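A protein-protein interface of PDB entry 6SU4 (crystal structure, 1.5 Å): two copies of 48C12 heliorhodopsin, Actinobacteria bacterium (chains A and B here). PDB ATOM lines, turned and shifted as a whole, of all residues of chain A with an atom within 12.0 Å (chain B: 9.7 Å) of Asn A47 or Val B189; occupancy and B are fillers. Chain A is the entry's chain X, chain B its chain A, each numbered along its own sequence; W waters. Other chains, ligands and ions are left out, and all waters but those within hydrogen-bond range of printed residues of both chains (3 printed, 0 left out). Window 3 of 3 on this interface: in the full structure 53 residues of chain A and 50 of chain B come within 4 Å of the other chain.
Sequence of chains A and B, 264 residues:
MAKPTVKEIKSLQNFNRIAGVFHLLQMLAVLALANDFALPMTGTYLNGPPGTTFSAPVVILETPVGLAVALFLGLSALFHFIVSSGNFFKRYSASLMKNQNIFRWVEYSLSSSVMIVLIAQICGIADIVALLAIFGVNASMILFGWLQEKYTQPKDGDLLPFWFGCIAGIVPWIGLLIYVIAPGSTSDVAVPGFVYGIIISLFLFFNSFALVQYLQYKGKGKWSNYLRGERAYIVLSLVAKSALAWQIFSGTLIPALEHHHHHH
Asn A47 touches one residue of chain B. Val B189 touches just these residues of chain A: Leu A46 (3.7 Å), Asn A47 (3.7 Å) and Gly A48 (3.7 Å). Gly A48 touches just one residue of chain B: Val B189. No residue of chain A comes within 4 Å of Ser B187. No residue of chain A comes within 4 Å of Ala B190. No residue of chain A comes within 4 Å of Val B191. Printed residues of chain A within 4 Å of Tyr B179: Gly A43 (3.6 Å), Thr A44 (2.9 Å) and Tyr A45 (3.7 Å). Printed residues of chain B within 4 Å of Pro A50: Ile B122 and Pro B192. Of the printed residues of chain A, Pro B192 touches Pro A50. Pro A57 touches none of the printed residues of chain B. The nearest residue of chain B that does not touch Asn A47 is Ser B187 (4.03 Å). The nearest residue of chain A that does not touch Val B189 is Ser A55 (5.0 Å). The nearest printed residue of chain A that does not touch Ile B122 is Leu A46 (4.03 Å).
Of the 17 printed residues of chain B, 8 touch a printed residue of chain A. Of the 16 printed residues of chain A, 9 touch a printed residue of chain B. Among the printed residues, 14 pairs touch across the chains. Among the printed residues, no Asp or Glu carboxylate lies within 4 Å of a Lys or Arg side-chain nitrogen of the other chain.
Among the printed residues, pairs that only touch across the chains: Phe A54 with Gly B124, Pro A50 with Ile B122, Tyr A45 with Ala B182, Leu A46 with Gly B124, Val A58 with Gly B184, Gly A43 with Tyr B179, Gly A48 with Val B189, Asn A47 with Val B189, Tyr A45 with Tyr B179, Thr A44 with Gly B124, Tyr A45 with Ser B185, Leu A46 with Val B189 and Pro A50 with Pro B192.
No position is printed for both chains.
N of Val A58 lies within hydrogen-bond range of O of Gly A43. O of Tyr A45 lies within hydrogen-bond range of N of Ser A55 (2.9 Å). The backbone carbonyl oxygen (O) of Thr A53 lies within hydrogen-bond range of the backbone NH (N) of Asn A47, 2.9 Å away. The backbone carbonyl oxygen of Ala B182 lies within hydrogen-bond range of the side-chain hydroxyl of Ser B185 (2.9 Å). O of Ser B187 sits at hydrogen-bond distance from OG of Ser B185, 3.0 Å away.
The backbone NH (N) of Thr A44 is in hydrogen-bond range of the side-chain hydroxyl (OH) of Tyr B179 (2.9 Å).
Water W3 lies within hydrogen-bond range of O of Thr A44 (2.7 Å) and O of Gly B124 (2.7 Å). Water W2 lies within hydrogen-bond range of OG of Ser A55 and OG1 of Thr B186. Water W1 bridges the backbone carbonyl oxygen (O) of Cys B123 (2.8 Å) and the backbone NH (N) of Leu A46 (2.9 Å).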
ATOM      1  N   GLY A  43     -23.945   7.886   7.220  1.00  0.00           N
ATOM      2  CA  GLY A  43     -25.026   8.879   7.276  1.00  0.00           C
ATOM      3  C   GLY A  43     -25.781   8.861   5.971  1.00  0.00           C
ATOM      4  O   GLY A  43     -25.128   8.836   4.916  1.00  0.00           O
ATOM      5  N   THR A  44     -27.109   8.808   6.039  1.00  0.00           N
ATOM      6  CA  THR A  44     -28.002   8.794   4.855  1.00  0.00           C
ATOM      7  C   THR A  44     -28.851  10.063   4.946  1.00  0.00           C
ATOM      8  O   THR A  44     -29.901  10.050   5.595  1.00  0.00           O
ATOM      9  CB  THR A  44     -28.790   7.480   4.762  1.00  0.00           C
ATOM     10  OG1 THR A  44     -27.868   6.387   4.803  1.00  0.00           O
ATOM     11  CG2 THR A  44     -29.605   7.390   3.491  1.00  0.00           C
ATOM     12  N   TYR A  45     -28.341  11.158   4.395  1.00  0.00           N
ATOM     13  CA  TYR A  45     -28.832  12.520   4.702  1.00  0.00           C
ATOM     14  C   TYR A  45     -29.931  12.908   3.721  1.00  0.00           C
ATOM     15  O   TYR A  45     -29.902  12.509   2.543  1.00  0.00           O
ATOM     16  CB  TYR A  45     -27.684  13.524   4.661  1.00  0.00           C
ATOM     17  CG  TYR A  45     -26.531  13.181   5.566  1.00  0.00           C
ATOM     18  CD1 TYR A  45     -26.732  12.946   6.916  1.00  0.00           C
ATOM     19  CD2 TYR A  45     -25.244  13.068   5.073  1.00  0.00           C
ATOM     20  CE1 TYR A  45     -25.679  12.627   7.755  1.00  0.00           C
ATOM     21  CE2 TYR A  45     -24.181  12.759   5.901  1.00  0.00           C
ATOM     22  CZ  TYR A  45     -24.398  12.531   7.248  1.00  0.00           C
ATOM     23  OH  TYR A  45     -23.355  12.227   8.079  1.00  0.00           O
ATOM     24  N   LEU A  46     -30.869  13.722   4.190  1.00  0.00           N
ATOM     25  CA  LEU A  46     -31.871  14.330   3.290  1.00  0.00           C
ATOM     26  C   LEU A  46     -31.144  15.119   2.199  1.00  0.00           C
ATOM     27  O   LEU A  46     -30.094  15.741   2.490  1.00  0.00           O
ATOM     28  CB  LEU A  46     -32.813  15.208   4.111  1.00  0.00           C
ATOM     29  CG  LEU A  46     -33.929  14.432   4.800  1.00  0.00           C
ATOM     30  CD1 LEU A  46     -34.596  15.276   5.868  1.00  0.00           C
ATOM     31  CD2 LEU A  46     -34.938  13.933   3.774  1.00  0.00           C
ATOM     32  N   ASN A  47     -31.681  15.062   0.982  1.00  0.00           N
ATOM     33  CA  ASN A  47     -31.159  15.779  -0.207  1.00  0.00           C
ATOM     34  C   ASN A  47     -32.137  16.904  -0.556  1.00  0.00           C
ATOM     35  O   ASN A  47     -32.132  17.373  -1.700  1.00  0.00           O
ATOM     36  CB  ASN A  47     -30.950  14.815  -1.375  1.00  0.00           C
ATOM     37  CG  ASN A  47     -29.983  15.346  -2.408  1.00  0.00           C
ATOM     38  OD1 ASN A  47     -29.961  14.867  -3.541  1.00  0.00           O
ATOM     39  ND2 ASN A  47     -29.183  16.328  -2.022  1.00  0.00           N
ATOM     40  N   GLY A  48     -32.947  17.290   0.425  1.00  0.00           N
ATOM     41  CA  GLY A  48     -33.969  18.345   0.348  1.00  0.00           C
ATOM     42  C   GLY A  48     -34.707  18.427   1.678  1.00  0.00           C
ATOM     43  O   GLY A  48     -34.245  17.880   2.683  1.00  0.00           O
ATOM     44  N   PRO A  49     -35.865  19.114   1.725  1.00  0.00           N
ATOM     45  CA  PRO A  49     -36.663  19.189   2.944  1.00  0.00           C
ATOM     46  C   PRO A  49     -37.171  17.826   3.405  1.00  0.00           C
ATOM     47  O   PRO A  49     -37.247  16.869   2.635  1.00  0.00           O
ATOM     48  CB  PRO A  49     -37.857  20.073   2.546  1.00  0.00           C
ATOM     49  CG  PRO A  49     -37.375  20.838   1.335  1.00  0.00           C
ATOM     50  CD  PRO A  49     -36.456  19.875   0.614  1.00  0.00           C
ATOM     51  N   PRO A  50     -37.572  17.699   4.683  1.00  0.00           N
ATOM     52  CA  PRO A  50     -38.160  16.458   5.164  1.00  0.00           C
ATOM     53  C   PRO A  50     -39.324  16.060   4.249  1.00  0.00           C
ATOM     54  O   PRO A  50     -40.075  16.929   3.848  1.00  0.00           O
ATOM     55  CB  PRO A  50     -38.655  16.763   6.586  1.00  0.00           C
ATOM     56  CG  PRO A  50     -38.006  18.080   6.976  1.00  0.00           C
ATOM     57  CD  PRO A  50     -37.494  18.740   5.715  1.00  0.00           C
ATOM     58  N   GLY A  51     -39.435  14.765   3.960  1.00  0.00           N
ATOM     59  CA  GLY A  51     -40.525  14.183   3.161  1.00  0.00           C
ATOM     60  C   GLY A  51     -40.202  14.188   1.681  1.00  0.00           C
ATOM     61  O   GLY A  51     -41.109  13.859   0.901  1.00  0.00           O
ATOM     62  N   THR A  52     -38.979  14.569   1.295  1.00  0.00           N
ATOM     63  CA  THR A  52     -38.529  14.528  -0.122  1.00  0.00           C
ATOM     64  C   THR A  52     -37.663  13.280  -0.315  1.00  0.00           C
ATOM     65  O   THR A  52     -38.185  12.167  -0.098  1.00  0.00           O
ATOM     66  CB  THR A  52     -37.880  15.843  -0.576  1.00  0.00           C
ATOM     67  OG1 THR A  52     -36.689  16.126   0.157  1.00  0.00           O
ATOM     68  CG2 THR A  52     -38.832  17.013  -0.444  1.00  0.00           C
ATOM     69  N   THR A  53     -36.410  13.447  -0.727  1.00  0.00           N
ATOM     70  CA  THR A  53     -35.531  12.315  -1.103  1.00  0.00           C
ATOM     71  C   THR A  53     -34.221  12.393  -0.325  1.00  0.00           C
ATOM     72  O   THR A  53     -33.935  13.454   0.276  1.00  0.00           O
ATOM     73  CB  THR A  53     -35.261  12.285  -2.608  1.00  0.00           C
ATOM     74  OG1 THR A  53     -34.433  13.414  -2.879  1.00  0.00           O
ATOM     75  CG2 THR A  53     -36.528  12.318  -3.430  1.00  0.00           C
ATOM     76  N   PHE A  54     -33.487  11.285  -0.327  1.00  0.00           N
ATOM     77  CA  PHE A  54     -32.217  11.119   0.418  1.00  0.00           C
ATOM     78  C   PHE A  54     -31.048  10.989  -0.555  1.00  0.00           C
ATOM     79  O   PHE A  54     -31.200  10.399  -1.642  1.00  0.00           O
ATOM     80  CB  PHE A  54     -32.284   9.885   1.322  1.00  0.00           C
ATOM     81  CG  PHE A  54     -33.241  10.021   2.475  1.00  0.00           C
ATOM     82  CD1 PHE A  54     -32.788  10.370   3.739  1.00  0.00           C
ATOM     83  CD2 PHE A  54     -34.601   9.824   2.293  1.00  0.00           C
ATOM     84  CE1 PHE A  54     -33.677  10.516   4.791  1.00  0.00           C
ATOM     85  CE2 PHE A  54     -35.485   9.958   3.352  1.00  0.00           C
ATOM     86  CZ  PHE A  54     -35.020  10.303   4.601  1.00  0.00           C
ATOM     87  N   SER A  55     -29.895  11.499  -0.137  1.00  0.00           N
ATOM     88  CA  SER A  55     -28.590  11.189  -0.765  1.00  0.00           C
ATOM     89  C   SER A  55     -28.290   9.709  -0.517  1.00  0.00           C
ATOM     90  O   SER A  55     -28.876   9.127   0.420  1.00  0.00           O
ATOM     91  CB  SER A  55     -27.508  12.099  -0.237  1.00  0.00           C
ATOM     92  OG  SER A  55     -27.773  13.449  -0.609  1.00  0.00           O
ATOM     93  N   ALA A  56     -27.416   9.113  -1.322  1.00  0.00           N
ATOM     94  CA  ALA A  56     -26.871   7.764  -1.067  1.00  0.00           C
ATOM     95  C   ALA A  56     -26.204   7.774   0.308  1.00  0.00           C
ATOM     96  O   ALA A  56     -25.644   8.796   0.716  1.00  0.00           O
ATOM     97  CB  ALA A  56     -25.887   7.404  -2.151  1.00  0.00           C
ATOM     98  N   PRO A  57     -26.203   6.644   1.045  1.00  0.00           N
ATOM     99  CA  PRO A  57     -25.439   6.557   2.285  1.00  0.00           C
ATOM    100  C   PRO A  57     -23.977   6.919   2.011  1.00  0.00           C
ATOM    101  O   PRO A  57     -23.445   6.523   0.981  1.00  0.00           O
ATOM    102  CB  PRO A  57     -25.577   5.092   2.722  1.00  0.00           C
ATOM    103  CG  PRO A  57     -26.824   4.602   2.011  1.00  0.00           C
ATOM    104  CD  PRO A  57     -26.871   5.377   0.708  1.00  0.00           C
ATOM    105  N   VAL A  58     -23.362   7.660   2.929  1.00  0.00           N
ATOM    106  CA  VAL A  58     -21.912   7.989   2.878  1.00  0.00           C
ATOM    107  C   VAL A  58     -21.243   7.379   4.111  1.00  0.00           C
ATOM    108  O   VAL A  58     -21.882   7.331   5.185  1.00  0.00           O
ATOM    109  CB  VAL A  58     -21.671   9.508   2.798  1.00  0.00           C
ATOM    110  CG1 VAL A  58     -22.316  10.109   1.562  1.00  0.00           C
ATOM    111  CG2 VAL A  58     -22.145  10.225   4.048  1.00  0.00           C
ATOM    112  N   ILE B 122     -37.759  14.084  11.328  1.00  0.00           N
ATOM    113  CA  ILE B 122     -37.808  15.439  10.707  1.00  0.00           C
ATOM    114  C   ILE B 122     -36.387  15.870  10.319  1.00  0.00           C
ATOM    115  O   ILE B 122     -36.227  16.584   9.311  1.00  0.00           O
ATOM    116  CB  ILE B 122     -38.536  16.421  11.641  1.00  0.00           C
ATOM    117  CG1 ILE B 122     -40.036  16.123  11.651  1.00  0.00           C
ATOM    118  CG2 ILE B 122     -38.235  17.862  11.253  1.00  0.00           C
ATOM    119  CD1 ILE B 122     -40.808  16.855  12.709  1.00  0.00           C
ATOM    120  N   CYS B 123     -35.368  15.411  11.046  1.00  0.00           N
ATOM    121  CA  CYS B 123     -33.947  15.715  10.751  1.00  0.00           C
ATOM    122  C   CYS B 123     -33.392  14.779   9.669  1.00  0.00           C
ATOM    123  O   CYS B 123     -32.233  14.971   9.284  1.00  0.00           O
ATOM    124  CB  CYS B 123     -33.089  15.604  12.005  1.00  0.00           C
ATOM    125  SG  CYS B 123     -33.399  16.922  13.209  1.00  0.00           S
ATOM    126  N   GLY B 124     -34.159  13.783   9.219  1.00  0.00           N
ATOM    127  CA  GLY B 124     -33.727  12.855   8.156  1.00  0.00           C
ATOM    128  C   GLY B 124     -33.204  11.529   8.678  1.00  0.00           C
ATOM    129  O   GLY B 124     -32.798  10.686   7.851  1.00  0.00           O
ATOM    130  N   TYR B 179     -26.584  14.448  12.421  1.00  0.00           N
ATOM    131  CA  TYR B 179     -27.375  14.496  11.167  1.00  0.00           C
ATOM    132  C   TYR B 179     -27.477  15.932  10.640  1.00  0.00           C
ATOM    133  O   TYR B 179     -27.476  16.087   9.408  1.00  0.00           O
ATOM    134  CB  TYR B 179     -28.722  13.786  11.321  1.00  0.00           C
ATOM    135  CG  TYR B 179     -28.690  12.442  10.643  1.00  0.00           C
ATOM    136  CD1 TYR B 179     -29.351  12.213   9.450  1.00  0.00           C
ATOM    137  CD2 TYR B 179     -27.874  11.431  11.135  1.00  0.00           C
ATOM    138  CE1 TYR B 179     -29.284  10.981   8.815  1.00  0.00           C
ATOM    139  CE2 TYR B 179     -27.789  10.201  10.507  1.00  0.00           C
ATOM    140  CZ  TYR B 179     -28.483   9.977   9.334  1.00  0.00           C
ATOM    141  OH  TYR B 179     -28.375   8.772   8.700  1.00  0.00           O
ATOM    142  N   VAL B 180     -27.530  16.945  11.507  1.00  0.00           N
ATOM    143  CA  VAL B 180     -27.617  18.361  11.041  1.00  0.00           C
ATOM    144  C   VAL B 180     -26.239  18.809  10.541  1.00  0.00           C
ATOM    145  O   VAL B 180     -26.195  19.528   9.527  1.00  0.00           O
ATOM    146  CB  VAL B 180     -28.207  19.306  12.107  1.00  0.00           C
ATOM    147  CG1 VAL B 180     -29.657  18.951  12.398  1.00  0.00           C
ATOM    148  CG2 VAL B 180     -27.391  19.334  13.383  1.00  0.00           C
ATOM    149  N   ILE B 181     -25.148  18.387  11.188  1.00  0.00           N
ATOM    150  CA  ILE B 181     -23.764  18.665  10.701  1.00  0.00           C
ATOM    151  C   ILE B 181     -23.525  17.891   9.397  1.00  0.00           C
ATOM    152  O   ILE B 181     -22.900  18.457   8.463  1.00  0.00           O
ATOM    153  CB  ILE B 181     -22.709  18.327  11.766  1.00  0.00           C
ATOM    154  CG1 ILE B 181     -22.859  19.211  13.009  1.00  0.00           C
ATOM    155  CG2 ILE B 181     -21.311  18.408  11.173  1.00  0.00           C
ATOM    156  CD1 ILE B 181     -22.014  18.767  14.179  1.00  0.00           C
ATOM    157  N   ALA B 182     -23.984  16.636   9.343  1.00  0.00           N
ATOM    158  CA  ALA B 182     -23.946  15.754   8.159  1.00  0.00           C
ATOM    159  C   ALA B 182     -22.503  15.562   7.708  1.00  0.00           C
ATOM    160  O   ALA B 182     -22.155  15.862   6.562  1.00  0.00           O
ATOM    161  CB  ALA B 182     -24.811  16.320   7.059  1.00  0.00           C
ATOM    162  N   GLY B 184     -19.237  14.043   6.101  1.00  0.00           N
ATOM    163  CA  GLY B 184     -18.993  13.227   4.896  1.00  0.00           C
ATOM    164  C   GLY B 184     -20.032  13.444   3.805  1.00  0.00           C
ATOM    165  O   GLY B 184     -19.961  12.742   2.781  1.00  0.00           O
ATOM    166  N   SER B 185     -20.974  14.366   3.988  1.00  0.00           N
ATOM    167  CA  SER B 185     -22.056  14.640   3.004  1.00  0.00           C
ATOM    168  C   SER B 185     -21.429  15.102   1.683  1.00  0.00           C
ATOM    169  O   SER B 185     -20.426  15.829   1.735  1.00  0.00           O
ATOM    170  CB  SER B 185     -23.034  15.645   3.529  1.00  0.00           C
ATOM    171  OG  SER B 185     -22.386  16.876   3.819  1.00  0.00           O
ATOM    172  N   THR B 186     -21.990  14.673   0.550  1.00  0.00           N
ATOM    173  CA  THR B 186     -21.492  15.006  -0.813  1.00  0.00           C
ATOM    174  C   THR B 186     -21.712  16.500  -1.079  1.00  0.00           C
ATOM    175  O   THR B 186     -20.860  17.114  -1.747  1.00  0.00           O
ATOM    176  CB  THR B 186     -22.171  14.128  -1.872  1.00  0.00           C
ATOM    177  OG1 THR B 186     -23.583  14.240  -1.686  1.00  0.00           O
ATOM    178  CG2 THR B 186     -21.744  12.679  -1.785  1.00  0.00           C
ATOM    179  N   SER B 187     -22.815  17.047  -0.564  1.00  0.00           N
ATOM    180  CA  SER B 187     -23.244  18.459  -0.741  1.00  0.00           C
ATOM    181  C   SER B 187     -23.581  19.069   0.623  1.00  0.00           C
ATOM    182  O   SER B 187     -23.788  18.295   1.576  1.00  0.00           O
ATOM    183  CB  SER B 187     -24.426  18.538  -1.671  1.00  0.00           C
ATOM    184  OG  SER B 187     -25.500  17.740  -1.188  1.00  0.00           O
ATOM    185  N   ASP B 188     -23.640  20.402   0.697  1.00  0.00           N
ATOM    186  CA  ASP B 188     -24.068  21.169   1.897  1.00  0.00           C
ATOM    187  C   ASP B 188     -25.570  21.452   1.792  1.00  0.00           C
ATOM    188  O   ASP B 188     -25.933  22.628   1.580  1.00  0.00           O
ATOM    189  CB  ASP B 188     -23.292  22.482   2.034  1.00  0.00           C
ATOM    190  CG  ASP B 188     -21.831  22.306   2.409  1.00  0.00           C
ATOM    191  OD1 ASP B 188     -21.503  21.272   3.024  1.00  0.00           O
ATOM    192  OD2 ASP B 188     -21.034  23.210   2.084  1.00  0.00           O
ATOM    193  N   VAL B 189     -26.406  20.420   1.932  1.00  0.00           N
ATOM    194  CA  VAL B 189     -27.892  20.539   1.845  1.00  0.00           C
ATOM    195  C   VAL B 189     -28.373  21.347   3.055  1.00  0.00           C
ATOM    196  O   VAL B 189     -27.954  21.031   4.185  1.00  0.00           O
ATOM    197  CB  VAL B 189     -28.582  19.164   1.765  1.00  0.00           C
ATOM    198  CG1 VAL B 189     -30.046  19.302   1.372  1.00  0.00           C
ATOM    199  CG2 VAL B 189     -27.860  18.219   0.815  1.00  0.00           C
ATOM    200  N   ALA B 190     -29.188  22.376   2.810  1.00  0.00           N
ATOM    201  CA  ALA B 190     -29.725  23.292   3.841  1.00  0.00           C
ATOM    202  C   ALA B 190     -30.775  22.556   4.679  1.00  0.00           C
ATOM    203  O   ALA B 190     -31.686  21.948   4.107  1.00  0.00           O
ATOM    204  CB  ALA B 190     -30.309  24.521   3.187  1.00  0.00           C
ATOM    205  N   VAL B 191     -30.623  22.590   6.000  1.00  0.00           N
ATOM    206  CA  VAL B 191     -31.676  22.167   6.964  1.00  0.00           C
ATOM    207  C   VAL B 191     -32.672  23.315   7.045  1.00  0.00           C
ATOM    208  O   VAL B 191     -32.261  24.447   7.280  1.00  0.00           O
ATOM    209  CB  VAL B 191     -31.058  21.862   8.340  1.00  0.00           C
ATOM    210  CG1 VAL B 191     -32.119  21.540   9.386  1.00  0.00           C
ATOM    211  CG2 VAL B 191     -30.014  20.764   8.247  1.00  0.00           C
ATOM    212  N   PRO B 192     -33.986  23.088   6.824  1.00  0.00           N
ATOM    213  CA  PRO B 192     -34.962  24.174   6.875  1.00  0.00           C
ATOM    214  C   PRO B 192     -34.974  24.877   8.239  1.00  0.00           C
ATOM    215  O   PRO B 192     -34.753  24.222   9.254  1.00  0.00           O
ATOM    216  CB  PRO B 192     -36.308  23.483   6.613  1.00  0.00           C
ATOM    217  CG  PRO B 192     -35.933  22.209   5.881  1.00  0.00           C
ATOM    218  CD  PRO B 192     -34.602  21.797   6.475  1.00  0.00           C
ATOM    219  N   TYR B 196     -34.563  23.617  12.454  1.00  0.00           N
ATOM    220  CA  TYR B 196     -33.725  24.238  13.510  1.00  0.00           C
ATOM    221  C   TYR B 196     -34.615  24.716  14.662  1.00  0.00           C
ATOM    222  O   TYR B 196     -34.239  24.520  15.821  1.00  0.00           O
ATOM    223  CB  TYR B 196     -32.870  25.369  12.934  1.00  0.00           C
ATOM    224  CG  TYR B 196     -31.670  24.891  12.160  1.00  0.00           C
ATOM    225  CD1 TYR B 196     -30.693  24.126  12.767  1.00  0.00           C
ATOM    226  CD2 TYR B 196     -31.493  25.237  10.831  1.00  0.00           C
ATOM    227  CE1 TYR B 196     -29.586  23.684  12.066  1.00  0.00           C
ATOM    228  CE2 TYR B 196     -30.385  24.816  10.119  1.00  0.00           C
ATOM    229  CZ  TYR B 196     -29.427  24.036  10.740  1.00  0.00           C
ATOM    230  OH  TYR B 196     -28.331  23.615  10.049  1.00  0.00           O
HETATM  231  O   HOH W   1     -30.610  14.616   6.980  1.00  0.00           O
HETATM  232  O   HOH W   2     -26.561  13.650  -3.159  1.00  0.00           O
HETATM  233  O   HOH W   3     -31.638   8.446   6.813  1.00  0.00           O
